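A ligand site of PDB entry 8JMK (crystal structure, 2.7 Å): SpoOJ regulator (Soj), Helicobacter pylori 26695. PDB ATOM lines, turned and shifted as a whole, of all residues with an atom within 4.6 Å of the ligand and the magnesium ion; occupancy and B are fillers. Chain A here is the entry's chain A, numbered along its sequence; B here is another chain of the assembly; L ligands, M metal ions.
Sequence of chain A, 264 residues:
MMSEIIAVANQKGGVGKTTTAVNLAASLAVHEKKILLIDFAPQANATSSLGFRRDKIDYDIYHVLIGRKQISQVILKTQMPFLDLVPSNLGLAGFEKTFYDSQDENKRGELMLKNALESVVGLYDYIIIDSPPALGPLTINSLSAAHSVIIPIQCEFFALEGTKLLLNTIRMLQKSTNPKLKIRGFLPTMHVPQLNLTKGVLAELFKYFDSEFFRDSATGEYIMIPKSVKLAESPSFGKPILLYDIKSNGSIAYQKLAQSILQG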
ATOM      1  N   LYS A  12      15.314 -18.337 -16.622  1.00  0.00           N
ATOM      2  CA  LYS A  12      14.025 -18.662 -17.216  1.00  0.00           C
ATOM      3  C   LYS A  12      14.286 -19.686 -18.297  1.00  0.00           C
ATOM      4  O   LYS A  12      15.247 -19.567 -19.065  1.00  0.00           O
ATOM      5  CB  LYS A  12      13.382 -17.425 -17.825  1.00  0.00           C
ATOM      6  CG  LYS A  12      11.932 -17.623 -18.207  1.00  0.00           C
ATOM      7  CD  LYS A  12      11.022 -17.894 -17.013  1.00  0.00           C
ATOM      8  CE  LYS A  12       9.647 -18.367 -17.485  1.00  0.00           C
ATOM      9  NZ  LYS A  12       9.663 -19.750 -18.105  1.00  0.00           N
ATOM     10  N   GLY A  13      13.447 -20.713 -18.330  1.00  0.00           N
ATOM     11  CA  GLY A  13      13.601 -21.704 -19.347  1.00  0.00           C
ATOM     12  C   GLY A  13      13.070 -21.296 -20.713  1.00  0.00           C
ATOM     13  O   GLY A  13      12.076 -20.569 -20.812  1.00  0.00           O
ATOM     14  N   GLY A  14      13.759 -21.753 -21.754  1.00  0.00           N
ATOM     15  CA  GLY A  14      13.255 -21.688 -23.103  1.00  0.00           C
ATOM     16  C   GLY A  14      13.083 -20.288 -23.653  1.00  0.00           C
ATOM     17  O   GLY A  14      12.096 -20.007 -24.319  1.00  0.00           O
ATOM     18  N   VAL A  15      14.024 -19.406 -23.325  1.00  0.00           N
ATOM     19  CA  VAL A  15      14.067 -18.021 -23.786  1.00  0.00           C
ATOM     20  C   VAL A  15      15.016 -17.708 -24.948  1.00  0.00           C
ATOM     21  O   VAL A  15      15.260 -16.533 -25.246  1.00  0.00           O
ATOM     22  CB  VAL A  15      14.353 -17.057 -22.620  1.00  0.00           C
ATOM     23  CG1 VAL A  15      13.320 -17.256 -21.559  1.00  0.00           C
ATOM     24  CG2 VAL A  15      15.767 -17.303 -22.054  1.00  0.00           C
ATOM     25  N   GLY A  16      15.638 -18.735 -25.527  1.00  0.00           N
ATOM     26  CA  GLY A  16      16.497 -18.502 -26.681  1.00  0.00           C
ATOM     27  C   GLY A  16      17.983 -18.437 -26.409  1.00  0.00           C
ATOM     28  O   GLY A  16      18.719 -18.035 -27.285  1.00  0.00           O
ATOM     29  N   LYS A  17      18.424 -18.853 -25.227  1.00  0.00           N
ATOM     30  CA  LYS A  17      19.843 -18.877 -24.847  1.00  0.00           C
ATOM     31  C   LYS A  17      20.687 -19.686 -25.803  1.00  0.00           C
ATOM     32  O   LYS A  17      21.743 -19.221 -26.203  1.00  0.00           O
ATOM     33  CB  LYS A  17      20.044 -19.459 -23.445  1.00  0.00           C
ATOM     34  CG  LYS A  17      19.285 -18.764 -22.354  1.00  0.00           C
ATOM     35  CD  LYS A  17      19.686 -19.263 -20.980  1.00  0.00           C
ATOM     36  CE  LYS A  17      19.188 -20.675 -20.676  1.00  0.00           C
ATOM     37  NZ  LYS A  17      17.755 -20.884 -20.903  1.00  0.00           N
ATOM     38  N   THR A  18      20.232 -20.867 -26.186  1.00  0.00           N
ATOM     39  CA  THR A  18      21.009 -21.720 -27.084  1.00  0.00           C
ATOM     40  C   THR A  18      20.947 -21.199 -28.506  1.00  0.00           C
ATOM     41  O   THR A  18      22.001 -21.037 -29.146  1.00  0.00           O
ATOM     42  CB  THR A  18      20.577 -23.187 -26.971  1.00  0.00           C
ATOM     43  OG1 THR A  18      21.200 -23.763 -25.817  1.00  0.00           O
ATOM     44  CG2 THR A  18      20.998 -23.988 -28.197  1.00  0.00           C
ATOM     45  N   THR A  19      19.731 -20.892 -28.980  1.00  0.00           N
ATOM     46  CA  THR A  19      19.538 -20.227 -30.263  1.00  0.00           C
ATOM     47  C   THR A  19      20.336 -18.925 -30.383  1.00  0.00           C
ATOM     48  O   THR A  19      20.905 -18.652 -31.427  1.00  0.00           O
ATOM     49  CB  THR A  19      18.038 -19.951 -30.524  1.00  0.00           C
ATOM     50  OG1 THR A  19      17.266 -21.097 -30.160  1.00  0.00           O
ATOM     51  CG2 THR A  19      17.792 -19.695 -31.984  1.00  0.00           C
ATOM     52  N   GLN A  43      21.465 -30.396 -20.740  1.00  0.00           N
ATOM     53  CA  GLN A  43      20.582 -30.870 -21.822  1.00  0.00           C
ATOM     54  C   GLN A  43      21.256 -30.867 -23.192  1.00  0.00           C
ATOM     55  O   GLN A  43      20.814 -31.563 -24.104  1.00  0.00           O
ATOM     56  CB  GLN A  43      19.286 -30.063 -21.884  1.00  0.00           C
ATOM     57  CG  GLN A  43      18.472 -30.064 -20.606  1.00  0.00           C
ATOM     58  CD  GLN A  43      18.740 -28.833 -19.771  1.00  0.00           C
ATOM     59  OE1 GLN A  43      19.900 -28.430 -19.603  1.00  0.00           O
ATOM     60  NE2 GLN A  43      17.666 -28.199 -19.277  1.00  0.00           N
ATOM     61  N   ASN A  45      21.785 -28.787 -25.881  1.00  0.00           N
ATOM     62  CA  ASN A  45      21.079 -28.464 -27.099  1.00  0.00           C
ATOM     63  C   ASN A  45      21.966 -27.673 -28.068  1.00  0.00           C
ATOM     64  O   ASN A  45      21.675 -27.608 -29.256  1.00  0.00           O
ATOM     65  CB  ASN A  45      19.795 -27.697 -26.811  1.00  0.00           C
ATOM     66  CG  ASN A  45      18.712 -28.576 -26.200  1.00  0.00           C
ATOM     67  OD1 ASN A  45      18.749 -29.819 -26.250  1.00  0.00           O
ATOM     68  ND2 ASN A  45      17.721 -27.930 -25.604  1.00  0.00           N
ATOM     69  N   ASP A 130      27.226 -21.149 -23.464  1.00  0.00           N
ATOM     70  CA  ASP A 130      25.776 -21.344 -23.368  1.00  0.00           C
ATOM     71  C   ASP A 130      25.431 -22.011 -22.046  1.00  0.00           C
ATOM     72  O   ASP A 130      25.777 -23.167 -21.831  1.00  0.00           O
ATOM     73  CB  ASP A 130      25.317 -22.205 -24.551  1.00  0.00           C
ATOM     74  CG  ASP A 130      23.796 -22.434 -24.590  1.00  0.00           C
ATOM     75  OD1 ASP A 130      23.029 -21.648 -23.977  1.00  0.00           O
ATOM     76  OD2 ASP A 130      23.371 -23.400 -25.269  1.00  0.00           O
ATOM     77  N   PRO A 133      19.251 -23.337 -17.752  1.00  0.00           N
ATOM     78  CA  PRO A 133      18.235 -22.510 -17.093  1.00  0.00           C
ATOM     79  C   PRO A 133      18.172 -22.535 -15.551  1.00  0.00           C
ATOM     80  O   PRO A 133      17.109 -22.836 -15.010  1.00  0.00           O
ATOM     81  CB  PRO A 133      16.918 -23.050 -17.667  1.00  0.00           C
ATOM     82  CG  PRO A 133      17.249 -24.394 -18.193  1.00  0.00           C
ATOM     83  CD  PRO A 133      18.635 -24.286 -18.702  1.00  0.00           C
ATOM     84  N   MET A 190      12.449 -14.138 -29.602  1.00  0.00           N
ATOM     85  CA  MET A 190      11.115 -14.645 -29.926  1.00  0.00           C
ATOM     86  C   MET A 190      10.146 -13.459 -30.041  1.00  0.00           C
ATOM     87  O   MET A 190       8.991 -13.533 -29.610  1.00  0.00           O
ATOM     88  CB  MET A 190      10.646 -15.736 -28.923  1.00  0.00           C
ATOM     89  CG  MET A 190      11.476 -17.030 -28.974  1.00  0.00           C
ATOM     90  SD  MET A 190      11.908 -17.881 -27.424  1.00  0.00           S
ATOM     91  CE  MET A 190      10.266 -18.418 -26.943  1.00  0.00           C
ATOM     92  N   ILE A 225      15.553 -10.305 -31.838  1.00  0.00           N
ATOM     93  CA  ILE A 225      15.368 -11.479 -32.687  1.00  0.00           C
ATOM     94  C   ILE A 225      13.892 -11.791 -32.816  1.00  0.00           C
ATOM     95  O   ILE A 225      13.215 -12.024 -31.811  1.00  0.00           O
ATOM     96  CB  ILE A 225      16.026 -12.692 -32.102  1.00  0.00           C
ATOM     97  CG1 ILE A 225      17.410 -12.341 -31.552  1.00  0.00           C
ATOM     98  CG2 ILE A 225      16.093 -13.796 -33.144  1.00  0.00           C
ATOM     99  CD1 ILE A 225      18.392 -11.920 -32.583  1.00  0.00           C
ATOM    100  N   PRO A 226      13.369 -11.793 -34.049  1.00  0.00           N
ATOM    101  CA  PRO A 226      11.926 -11.993 -34.249  1.00  0.00           C
ATOM    102  C   PRO A 226      11.547 -13.452 -34.143  1.00  0.00           C
ATOM    103  O   PRO A 226      12.379 -14.317 -34.330  1.00  0.00           O
ATOM    104  CB  PRO A 226      11.708 -11.530 -35.693  1.00  0.00           C
ATOM    105  CG  PRO A 226      13.025 -11.778 -36.348  1.00  0.00           C
ATOM    106  CD  PRO A 226      14.093 -11.641 -35.320  1.00  0.00           C
ATOM    107  N   LYS A 227      10.290 -13.696 -33.843  1.00  0.00           N
ATOM    108  CA  LYS A 227       9.802 -15.036 -33.794  1.00  0.00           C
ATOM    109  C   LYS A 227       9.748 -15.556 -35.233  1.00  0.00           C
ATOM    110  O   LYS A 227       9.015 -15.044 -36.080  1.00  0.00           O
ATOM    111  CB  LYS A 227       8.414 -15.043 -33.175  1.00  0.00           C
ATOM    112  CG  LYS A 227       8.043 -16.352 -32.563  1.00  0.00           C
ATOM    113  CD  LYS A 227       6.553 -16.489 -32.424  1.00  0.00           C
ATOM    114  CE  LYS A 227       6.146 -17.906 -32.753  1.00  0.00           C
ATOM    115  NZ  LYS A 227       6.463 -18.153 -34.216  1.00  0.00           N
ATOM    116  N   SER A 228      10.526 -16.586 -35.503  1.00  0.00           N
ATOM    117  CA  SER A 228      10.675 -17.137 -36.841  1.00  0.00           C
ATOM    118  C   SER A 228      10.793 -18.630 -36.632  1.00  0.00           C
ATOM    119  O   SER A 228      11.665 -19.063 -35.887  1.00  0.00           O
ATOM    120  CB  SER A 228      11.978 -16.617 -37.475  1.00  0.00           C
ATOM    121  OG  SER A 228      12.185 -17.067 -38.794  1.00  0.00           O
ATOM    122  N   LEU A 231      14.132 -20.522 -37.245  1.00  0.00           N
ATOM    123  CA  LEU A 231      15.157 -20.510 -36.211  1.00  0.00           C
ATOM    124  C   LEU A 231      15.003 -21.784 -35.426  1.00  0.00           C
ATOM    125  O   LEU A 231      15.971 -22.310 -34.861  1.00  0.00           O
ATOM    126  CB  LEU A 231      14.900 -19.348 -35.254  1.00  0.00           C
ATOM    127  CG  LEU A 231      15.865 -18.175 -35.128  1.00  0.00           C
ATOM    128  CD1 LEU A 231      16.817 -18.105 -36.261  1.00  0.00           C
ATOM    129  CD2 LEU A 231      15.038 -16.922 -35.074  1.00  0.00           C
ATOM    130  N   ALA A 232      13.764 -22.253 -35.387  1.00  0.00           N
ATOM    131  CA  ALA A 232      13.370 -23.452 -34.699  1.00  0.00           C
ATOM    132  C   ALA A 232      13.646 -24.724 -35.512  1.00  0.00           C
ATOM    133  O   ALA A 232      14.015 -25.766 -34.962  1.00  0.00           O
ATOM    134  CB  ALA A 232      11.956 -23.366 -34.399  1.00  0.00           C
ATOM    135  N   PRO A 235      18.056 -26.035 -36.060  1.00  0.00           N
ATOM    136  CA  PRO A 235      18.830 -27.104 -35.418  1.00  0.00           C
ATOM    137  C   PRO A 235      18.455 -28.552 -35.838  1.00  0.00           C
ATOM    138  O   PRO A 235      19.317 -29.425 -35.677  1.00  0.00           O
ATOM    139  CB  PRO A 235      18.485 -26.916 -33.945  1.00  0.00           C
ATOM    140  CG  PRO A 235      17.107 -26.361 -33.972  1.00  0.00           C
ATOM    141  CD  PRO A 235      17.236 -25.343 -35.044  1.00  0.00           C
ATOM    142  N   LYS B  12      13.336 -29.660 -20.327  1.00  0.00           N
ATOM    143  CA  LYS B  12      13.490 -28.593 -21.286  1.00  0.00           C
ATOM    144  C   LYS B  12      12.848 -27.364 -20.704  1.00  0.00           C
ATOM    145  O   LYS B  12      11.782 -27.429 -20.089  1.00  0.00           O
ATOM    146  CB  LYS B  12      12.815 -28.949 -22.637  1.00  0.00           C
ATOM    147  CG  LYS B  12      12.989 -27.925 -23.751  1.00  0.00           C
ATOM    148  CD  LYS B  12      14.470 -27.709 -24.155  1.00  0.00           C
ATOM    149  CE  LYS B  12      14.640 -26.710 -25.284  1.00  0.00           C
ATOM    150  NZ  LYS B  12      13.889 -25.475 -24.997  1.00  0.00           N
ATOM    151  N   GLY B  13      13.514 -26.229 -20.856  1.00  0.00           N
ATOM    152  CA  GLY B  13      12.970 -25.015 -20.347  1.00  0.00           C
ATOM    153  C   GLY B  13      11.859 -24.432 -21.215  1.00  0.00           C
ATOM    154  O   GLY B  13      11.852 -24.585 -22.442  1.00  0.00           O
ATOM    155  N   GLN B 154       6.295 -28.958 -25.920  1.00  0.00           N
ATOM    156  CA  GLN B 154       6.358 -27.844 -26.836  1.00  0.00           C
ATOM    157  C   GLN B 154       6.767 -28.568 -28.115  1.00  0.00           C
ATOM    158  O   GLN B 154       7.764 -29.281 -28.097  1.00  0.00           O
ATOM    159  CB  GLN B 154       7.455 -26.891 -26.357  1.00  0.00           C
ATOM    160  CG  GLN B 154       7.432 -25.465 -26.854  1.00  0.00           C
ATOM    161  CD  GLN B 154       8.822 -24.864 -26.876  1.00  0.00           C
ATOM    162  OE1 GLN B 154       9.824 -25.604 -26.970  1.00  0.00           O
ATOM    163  NE2 GLN B 154       8.913 -23.546 -26.754  1.00  0.00           N
ATOM    164  N   GLU B 156       8.517 -29.026 -30.961  1.00  0.00           N
ATOM    165  CA  GLU B 156       9.648 -28.346 -31.598  1.00  0.00           C
ATOM    166  C   GLU B 156      10.829 -29.293 -31.426  1.00  0.00           C
ATOM    167  O   GLU B 156      10.668 -30.294 -30.737  1.00  0.00           O
ATOM    168  CB  GLU B 156       9.910 -26.951 -30.965  1.00  0.00           C
ATOM    169  CG  GLU B 156       8.932 -25.834 -31.438  1.00  0.00           C
ATOM    170  CD  GLU B 156       9.188 -24.500 -30.831  1.00  0.00           C
ATOM    171  OE1 GLU B 156      10.347 -24.255 -30.476  1.00  0.00           O
ATOM    172  OE2 GLU B 156       8.215 -23.700 -30.715  1.00  0.00           O
ATOM    173  N   PHE B 158      13.833 -29.989 -29.986  1.00  0.00           N
ATOM    174  CA  PHE B 158      14.630 -30.516 -28.901  1.00  0.00           C
ATOM    175  C   PHE B 158      13.839 -31.466 -28.055  1.00  0.00           C
ATOM    176  O   PHE B 158      14.416 -32.251 -27.301  1.00  0.00           O
ATOM    177  CB  PHE B 158      15.220 -29.390 -28.054  1.00  0.00           C
ATOM    178  CG  PHE B 158      16.200 -28.535 -28.802  1.00  0.00           C
ATOM    179  CD1 PHE B 158      17.382 -29.086 -29.299  1.00  0.00           C
ATOM    180  CD2 PHE B 158      15.922 -27.192 -29.025  1.00  0.00           C
ATOM    181  CE1 PHE B 158      18.299 -28.296 -29.991  1.00  0.00           C
ATOM    182  CE2 PHE B 158      16.801 -26.396 -29.732  1.00  0.00           C
ATOM    183  CZ  PHE B 158      18.009 -26.942 -30.211  1.00  0.00           C
HETATM  184  P1  LIG L   1      16.601 -24.057 -22.228  1.00  0.00           P
HETATM  185  O1  LIG L   1      18.063 -23.745 -22.226  1.00  0.00           O
HETATM  186  O2  LIG L   1      16.217 -25.520 -22.412  1.00  0.00           O
HETATM  187  O3  LIG L   1      15.893 -23.359 -21.098  1.00  0.00           O
HETATM  188  P2  LIG L   1      16.922 -22.014 -24.131  1.00  0.00           P
HETATM  189  O4  LIG L   1      18.203 -22.504 -24.726  1.00  0.00           O
HETATM  190  O5  LIG L   1      16.925 -20.860 -23.160  1.00  0.00           O
HETATM  191  O6  LIG L   1      16.075 -23.247 -23.529  1.00  0.00           O
HETATM  192  P3  LIG L   1      16.116 -22.214 -26.769  1.00  0.00           P
HETATM  193  O7  LIG L   1      17.242 -21.582 -27.547  1.00  0.00           O
HETATM  194  O8  LIG L   1      16.075 -23.717 -26.623  1.00  0.00           O
HETATM  195  O9  LIG L   1      15.982 -21.529 -25.317  1.00  0.00           O
HETATM  196  O10 LIG L   1      14.704 -21.788 -27.363  1.00  0.00           O
HETATM  197  C1  LIG L   1      13.599 -22.545 -26.924  1.00  0.00           C
HETATM  198  C2  LIG L   1      12.971 -23.002 -28.225  1.00  0.00           C
HETATM  199  O11 LIG L   1      12.770 -21.851 -29.011  1.00  0.00           O
HETATM  200  C3  LIG L   1      13.849 -23.889 -29.098  1.00  0.00           C
HETATM  201  O12 LIG L   1      12.982 -24.966 -29.468  1.00  0.00           O
HETATM  202  C4  LIG L   1      14.191 -23.062 -30.321  1.00  0.00           C
HETATM  203  O13 LIG L   1      14.340 -23.907 -31.469  1.00  0.00           O
HETATM  204  C5  LIG L   1      12.885 -22.313 -30.335  1.00  0.00           C
HETATM  205  N1  LIG L   1      12.591 -21.146 -31.168  1.00  0.00           N
HETATM  206  C6  LIG L   1      11.534 -21.017 -32.006  1.00  0.00           C
HETATM  207  N2  LIG L   1      11.458 -19.804 -32.604  1.00  0.00           N
HETATM  208  C7  LIG L   1      12.476 -19.142 -32.051  1.00  0.00           C
HETATM  209  C8  LIG L   1      12.970 -17.790 -32.192  1.00  0.00           C
HETATM  210  N3  LIG L   1      12.317 -17.014 -33.069  1.00  0.00           N
HETATM  211  N4  LIG L   1      14.055 -17.436 -31.455  1.00  0.00           N
HETATM  212  C9  LIG L   1      14.659 -18.293 -30.600  1.00  0.00           C
HETATM  213  N5  LIG L   1      14.255 -19.572 -30.398  1.00  0.00           N
HETATM  214  C10 LIG L   1      13.198 -20.009 -31.097  1.00  0.00           C
HETATM  215 MG    MG M   1      19.181 -24.372 -24.129  1.00  0.00          MG
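An oxygen (O5) of the ligand is in hydrogen-bond range of the backbone NH (N) of Lys 17, 3.2 Å away. N of Thr 19 is in hydrogen-bond range of O7 of the ligand. The side-chain hydroxyl of Thr 18 lies close to an oxygen (O4) of the ligand, at 3.4 Å. The backbone NH of Val 15 lies within hydrogen-bond range of an oxygen (O5) of the ligand, 3.2 Å away. The backbone NH of Thr 18 sits at hydrogen-bond distance from an oxygen (O7) of the ligand (3.4 Å). The backbone NH of Gly 13 of chain B is in hydrogen-bond range of an oxygen (O2) of the ligand (3.2 Å). The side-chain hydroxyl of Thr 19 sits at hydrogen-bond distance from an oxygen (O7) of the ligand, at 2.7 Å. O3 of the ligand is in hydrogen-bond range of N of Gly 14 (2.8 Å). O5 of the ligand lies within salt-bridge range of NZ of Lys 17, at 2.4 Å. NZ of Lys 12 of chain B is in salt-bridge range of O8 of the ligand. The backbone carbonyl oxygen (O) of Pro 226 is in hydrogen-bond range of a nitrogen (N3) of the ligand. The backbone NH (N) of Gly 16 sits at hydrogen-bond distance from an oxygen (O9) of the ligand (2.8 Å). O12 of the ligand is in hydrogen-bond range of OE1 of Glu 156 of chain B, at 2.9 Å.
The side-chain hydroxyl of Thr 18 sits close to the side-chain carboxylate of Asp 130. The backbone NH (N) of Met 190 is in hydrogen-bond range of the backbone carbonyl oxygen (O) of Ile 225, 3.2 Å away. The backbone NH of Gly 14 sits close to the backbone carbonyl oxygen of Gly 13 of chain B, 3.5 Å away. NZ of Lys 17 sits at hydrogen-bond distance from O of Lys 12 of chain A (3.4 Å).
The backbone NH (N) of Ser 228 sits close to a nitrogen (N3) of the ligand (3.1 Å). Merely in contact with the ligand: Lys 227, Gly 13 of chain A, Pro 133, Ala 232, Leu 231, Met 190 and Phe 158 of chain B. Hydrophobic or aromatic side chains that line the ligand: Val 15, Pro 133, Met 190, Leu 231, Ala 232 and Phe 158 of chain B. 18 residues have an atom within 4 Å of the ligand: Gly 13 of chain A, Gly 14, Val 15, Gly 16, Lys 17, Thr 18, Thr 19, Pro 133, Met 190, Pro 226, Lys 227, Ser 228, Leu 231, Ala 232, Lys 12 of chain B, Gly 13 of chain B, Glu 156 of chain B and Phe 158 of chain B. The nearest printed residue that does not touch the ligand is Gln 154 of chain B (4.1 Å).
One residue has an atom within 4 Å of the magnesium ion: Thr 18.
The magnesium ion is bound by an oxygen (O4) of the ligand and an oxygen (O1) of the ligand. Slightly farther from the magnesium ion lies OG1 of Thr 18 (2.7 Å).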
